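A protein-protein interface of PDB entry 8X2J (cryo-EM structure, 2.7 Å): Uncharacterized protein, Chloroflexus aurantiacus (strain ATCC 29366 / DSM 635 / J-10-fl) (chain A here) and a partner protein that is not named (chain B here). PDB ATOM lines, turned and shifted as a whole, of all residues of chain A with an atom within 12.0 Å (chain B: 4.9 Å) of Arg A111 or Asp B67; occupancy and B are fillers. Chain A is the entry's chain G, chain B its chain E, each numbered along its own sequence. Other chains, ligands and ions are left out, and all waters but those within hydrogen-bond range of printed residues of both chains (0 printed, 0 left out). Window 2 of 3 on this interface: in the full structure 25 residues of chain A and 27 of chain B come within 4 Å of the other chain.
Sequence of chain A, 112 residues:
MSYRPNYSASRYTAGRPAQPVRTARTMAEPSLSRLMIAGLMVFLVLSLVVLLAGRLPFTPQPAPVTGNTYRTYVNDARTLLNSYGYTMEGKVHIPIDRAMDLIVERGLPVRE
The side-chain carboxylate of Asp B67 lies within salt-bridge range of the guanidinium group of Arg A111 (3.1 Å).
N of Met B83 lies within hydrogen-bond range of O of Pro A109 (2.9 Å).
The backbone carbonyl oxygen of Met B83 is in hydrogen-bond range of the backbone NH of Arg A111 (3.2 Å).
Among the printed residues, merely in contact across the chains: Leu A108 with Met B83 (3.7 Å), Pro A109 with Ala B82 (3.4 Å), Val A110 with Met B83 (3.3 Å), Arg A111 with Phe B69 (3.4 Å), Arg A111 with Val B80 (3.5 Å) and Arg A111 with Ala B82 (3.4 Å).
Printed residues of chain A that touch a printed residue of chain B: Leu A108, Pro A109, Val A110 and Arg A111.
Of the 11 printed residues of chain B, 5 touch a printed residue of chain A.
Hydrophobic or aromatic side chains of chain B that line the printed part of chain A: Phe B69, Val B80, Ala B82 and Met B83.
Among the printed residues, 9 pairs touch across the chains.
Gly A107 touches none of the printed residues of chain B.
Of the printed residues of chain B, Leu A108 touches Met B83 (3.7 Å).
Of the printed residues of chain B, Val A110 touches Met B83 (3.3 Å).
Of chain B, only Asp B67, Phe B69, Val B80, Ala B82 and Met B83 come within 4 Å of Arg A111.
Lys B65 touches none of the printed residues of chain A.
No residue of chain A comes within 4 Å of Thr B66.
Of the printed residues of chain A, Asp B67 touches Arg A111.
No residue of chain A comes within 4 Å of Glu B68.
Tyr B71 touches none of the printed residues of chain A.
Of chain A, only Arg A111 comes within 4 Å of Val B80.
Printed residues of chain A within 4 Å of Ala B82: Pro A109 and Arg A111.
Printed residues of chain A within 4 Å of Met B83: Leu A108 (3.7 Å), Pro A109 (2.9 Å), Val A110 (3.3 Å) and Arg A111 (3.2 Å).
No residue of chain A comes within 4 Å of Pro B84.
The nearest residue of chain B that does not touch Arg A111 is Pro B84 (4.6 Å).
The nearest residue of chain A that does not touch Asp B67 is Val A110 (9.1 Å).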
ATOM      1  N   GLY A 107      11.827  -8.275  -7.102  1.00  0.00           N
ATOM      2  CA  GLY A 107      13.177  -8.768  -7.259  1.00  0.00           C
ATOM      3  C   GLY A 107      14.191  -7.967  -6.466  1.00  0.00           C
ATOM      4  O   GLY A 107      13.888  -6.977  -5.799  1.00  0.00           O
ATOM      5  N   LEU A 108      15.434  -8.426  -6.548  1.00  0.00           N
ATOM      6  CA  LEU A 108      16.582  -7.768  -5.950  1.00  0.00           C
ATOM      7  C   LEU A 108      17.709  -7.721  -6.969  1.00  0.00           C
ATOM      8  O   LEU A 108      17.753  -8.556  -7.878  1.00  0.00           O
ATOM      9  CB  LEU A 108      17.042  -8.508  -4.683  1.00  0.00           C
ATOM     10  CG  LEU A 108      16.192  -8.264  -3.433  1.00  0.00           C
ATOM     11  CD1 LEU A 108      16.747  -9.025  -2.240  1.00  0.00           C
ATOM     12  CD2 LEU A 108      16.096  -6.777  -3.125  1.00  0.00           C
ATOM     13  N   PRO A 109      18.604  -6.731  -6.877  1.00  0.00           N
ATOM     14  CA  PRO A 109      19.757  -6.700  -7.790  1.00  0.00           C
ATOM     15  C   PRO A 109      20.693  -7.877  -7.563  1.00  0.00           C
ATOM     16  O   PRO A 109      20.955  -8.280  -6.427  1.00  0.00           O
ATOM     17  CB  PRO A 109      20.441  -5.367  -7.457  1.00  0.00           C
ATOM     18  CG  PRO A 109      19.910  -4.977  -6.117  1.00  0.00           C
ATOM     19  CD  PRO A 109      18.514  -5.497  -6.079  1.00  0.00           C
ATOM     20  N   VAL A 110      21.187  -8.434  -8.666  1.00  0.00           N
ATOM     21  CA  VAL A 110      22.030  -9.623  -8.655  1.00  0.00           C
ATOM     22  C   VAL A 110      23.357  -9.273  -9.313  1.00  0.00           C
ATOM     23  O   VAL A 110      23.374  -8.758 -10.438  1.00  0.00           O
ATOM     24  CB  VAL A 110      21.350 -10.804  -9.375  1.00  0.00           C
ATOM     25  CG1 VAL A 110      22.285 -11.999  -9.460  1.00  0.00           C
ATOM     26  CG2 VAL A 110      20.065 -11.193  -8.661  1.00  0.00           C
ATOM     27  N   ARG A 111      24.455  -9.552  -8.602  1.00  0.00           N
ATOM     28  CA  ARG A 111      25.840  -9.308  -9.032  1.00  0.00           C
ATOM     29  C   ARG A 111      26.104  -7.854  -9.425  1.00  0.00           C
ATOM     30  O   ARG A 111      26.849  -7.144  -8.749  1.00  0.00           O
ATOM     31  CB  ARG A 111      26.219 -10.237 -10.192  1.00  0.00           C
ATOM     32  CG  ARG A 111      26.023 -11.711  -9.889  1.00  0.00           C
ATOM     33  CD  ARG A 111      27.125 -12.240  -8.988  1.00  0.00           C
ATOM     34  NE  ARG A 111      28.435 -12.152  -9.623  1.00  0.00           N
ATOM     35  CZ  ARG A 111      29.578 -12.459  -9.027  1.00  0.00           C
ATOM     36  NH1 ARG A 111      29.611 -12.886  -7.775  1.00  0.00           N
ATOM     37  NH2 ARG A 111      30.716 -12.340  -9.705  1.00  0.00           N
ATOM     38  N   LYS B  65      35.196 -22.087  -2.363  1.00  0.00           N
ATOM     39  CA  LYS B  65      35.226 -20.717  -1.865  1.00  0.00           C
ATOM     40  C   LYS B  65      35.602 -19.720  -2.956  1.00  0.00           C
ATOM     41  O   LYS B  65      36.089 -18.628  -2.649  1.00  0.00           O
ATOM     42  CB  LYS B  65      36.201 -20.598  -0.693  1.00  0.00           C
ATOM     43  CG  LYS B  65      36.012 -21.627   0.408  1.00  0.00           C
ATOM     44  CD  LYS B  65      34.921 -21.209   1.376  1.00  0.00           C
ATOM     45  CE  LYS B  65      34.753 -22.224   2.494  1.00  0.00           C
ATOM     46  NZ  LYS B  65      35.944 -22.268   3.387  1.00  0.00           N
ATOM     47  N   THR B  66      35.392 -20.077  -4.225  1.00  0.00           N
ATOM     48  CA  THR B  66      35.840 -19.232  -5.327  1.00  0.00           C
ATOM     49  C   THR B  66      34.976 -17.990  -5.498  1.00  0.00           C
ATOM     50  O   THR B  66      35.481 -16.946  -5.929  1.00  0.00           O
ATOM     51  CB  THR B  66      35.856 -20.025  -6.631  1.00  0.00           C
ATOM     52  OG1 THR B  66      34.649 -20.786  -6.743  1.00  0.00           O
ATOM     53  CG2 THR B  66      37.043 -20.964  -6.650  1.00  0.00           C
ATOM     54  N   ASP B  67      33.688 -18.080  -5.184  1.00  0.00           N
ATOM     55  CA  ASP B  67      32.802 -16.923  -5.260  1.00  0.00           C
ATOM     56  C   ASP B  67      33.115 -16.005  -4.088  1.00  0.00           C
ATOM     57  O   ASP B  67      32.702 -16.259  -2.955  1.00  0.00           O
ATOM     58  CB  ASP B  67      31.342 -17.362  -5.251  1.00  0.00           C
ATOM     59  CG  ASP B  67      30.398 -16.263  -5.705  1.00  0.00           C
ATOM     60  OD1 ASP B  67      30.884 -15.213  -6.173  1.00  0.00           O
ATOM     61  OD2 ASP B  67      29.168 -16.450  -5.598  1.00  0.00           O
ATOM     62  N   GLU B  68      33.871 -14.937  -4.361  1.00  0.00           N
ATOM     63  CA  GLU B  68      34.233 -13.993  -3.311  1.00  0.00           C
ATOM     64  C   GLU B  68      33.030 -13.190  -2.838  1.00  0.00           C
ATOM     65  O   GLU B  68      32.967 -12.811  -1.664  1.00  0.00           O
ATOM     66  CB  GLU B  68      35.336 -13.057  -3.803  1.00  0.00           C
ATOM     67  CG  GLU B  68      36.603 -13.774  -4.237  1.00  0.00           C
ATOM     68  CD  GLU B  68      37.348 -14.399  -3.072  1.00  0.00           C
ATOM     69  OE1 GLU B  68      37.495 -13.726  -2.030  1.00  0.00           O
ATOM     70  OE2 GLU B  68      37.781 -15.563  -3.198  1.00  0.00           O
ATOM     71  N   PHE B  69      32.067 -12.931  -3.726  1.00  0.00           N
ATOM     72  CA  PHE B  69      30.864 -12.207  -3.329  1.00  0.00           C
ATOM     73  C   PHE B  69      29.965 -13.049  -2.431  1.00  0.00           C
ATOM     74  O   PHE B  69      29.188 -12.497  -1.643  1.00  0.00           O
ATOM     75  CB  PHE B  69      30.095 -11.747  -4.566  1.00  0.00           C
ATOM     76  CG  PHE B  69      29.003 -10.764  -4.268  1.00  0.00           C
ATOM     77  CD1 PHE B  69      29.226  -9.703  -3.408  1.00  0.00           C
ATOM     78  CD2 PHE B  69      27.750 -10.905  -4.844  1.00  0.00           C
ATOM     79  CE1 PHE B  69      28.221  -8.797  -3.129  1.00  0.00           C
ATOM     80  CE2 PHE B  69      26.741 -10.001  -4.570  1.00  0.00           C
ATOM     81  CZ  PHE B  69      26.979  -8.945  -3.712  1.00  0.00           C
ATOM     82  N   LEU B  70      30.058 -14.377  -2.531  1.00  0.00           N
ATOM     83  CA  LEU B  70      29.255 -15.247  -1.680  1.00  0.00           C
ATOM     84  C   LEU B  70      29.757 -15.257  -0.241  1.00  0.00           C
ATOM     85  O   LEU B  70      28.958 -15.414   0.689  1.00  0.00           O
ATOM     86  CB  LEU B  70      29.251 -16.668  -2.246  1.00  0.00           C
ATOM     87  CG  LEU B  70      28.302 -17.706  -1.646  1.00  0.00           C
ATOM     88  CD1 LEU B  70      26.856 -17.279  -1.806  1.00  0.00           C
ATOM     89  CD2 LEU B  70      28.537 -19.062  -2.284  1.00  0.00           C
ATOM     90  N   TYR B  71      31.063 -15.085  -0.034  1.00  0.00           N
ATOM     91  CA  TYR B  71      31.653 -15.208   1.291  1.00  0.00           C
ATOM     92  C   TYR B  71      32.095 -13.885   1.898  1.00  0.00           C
ATOM     93  O   TYR B  71      32.389 -13.845   3.098  1.00  0.00           O
ATOM     94  CB  TYR B  71      32.841 -16.179   1.249  1.00  0.00           C
ATOM     95  CG  TYR B  71      32.417 -17.606   0.995  1.00  0.00           C
ATOM     96  CD1 TYR B  71      32.003 -18.422   2.040  1.00  0.00           C
ATOM     97  CD2 TYR B  71      32.408 -18.130  -0.292  1.00  0.00           C
ATOM     98  CE1 TYR B  71      31.605 -19.727   1.814  1.00  0.00           C
ATOM     99  CE2 TYR B  71      32.010 -19.433  -0.530  1.00  0.00           C
ATOM    100  CZ  TYR B  71      31.611 -20.225   0.527  1.00  0.00           C
ATOM    101  OH  TYR B  71      31.215 -21.523   0.297  1.00  0.00           O
ATOM    102  N   VAL B  80      28.771  -3.282  -3.053  1.00  0.00           N
ATOM    103  CA  VAL B  80      28.242  -3.825  -4.295  1.00  0.00           C
ATOM    104  C   VAL B  80      26.762  -3.502  -4.477  1.00  0.00           C
ATOM    105  O   VAL B  80      26.346  -3.130  -5.578  1.00  0.00           O
ATOM    106  CB  VAL B  80      28.485  -5.347  -4.370  1.00  0.00           C
ATOM    107  CG1 VAL B  80      28.228  -5.861  -5.777  1.00  0.00           C
ATOM    108  CG2 VAL B  80      29.901  -5.673  -3.933  1.00  0.00           C
ATOM    109  N   ALA B  82      24.137  -5.819  -4.159  1.00  0.00           N
ATOM    110  CA  ALA B  82      23.672  -6.892  -5.027  1.00  0.00           C
ATOM    111  C   ALA B  82      23.490  -8.151  -4.188  1.00  0.00           C
ATOM    112  O   ALA B  82      23.602  -8.122  -2.959  1.00  0.00           O
ATOM    113  CB  ALA B  82      24.649  -7.107  -6.189  1.00  0.00           C
ATOM    114  N   MET B  83      23.207  -9.266  -4.861  1.00  0.00           N
ATOM    115  CA  MET B  83      22.986 -10.551  -4.223  1.00  0.00           C
ATOM    116  C   MET B  83      23.560 -11.649  -5.107  1.00  0.00           C
ATOM    117  O   MET B  83      23.420 -11.584  -6.337  1.00  0.00           O
ATOM    118  CB  MET B  83      21.492 -10.800  -3.981  1.00  0.00           C
ATOM    119  CG  MET B  83      21.186 -11.619  -2.744  1.00  0.00           C
ATOM    120  SD  MET B  83      19.442 -11.610  -2.307  1.00  0.00           S
ATOM    121  CE  MET B  83      19.487 -12.589  -0.814  1.00  0.00           C
ATOM    122  N   PRO B  84      24.223 -12.654  -4.524  1.00  0.00           N
ATOM    123  CA  PRO B  84      24.765 -13.749  -5.348  1.00  0.00           C
ATOM    124  C   PRO B  84      23.706 -14.654  -5.960  1.00  0.00           C
ATOM    125  O   PRO B  84      24.012 -15.364  -6.924  1.00  0.00           O
ATOM    126  CB  PRO B  84      25.654 -14.522  -4.364  1.00  0.00           C
ATOM    127  CG  PRO B  84      25.129 -14.168  -3.018  1.00  0.00           C
ATOM    128  CD  PRO B  84      24.657 -12.755  -3.122  1.00  0.00           C
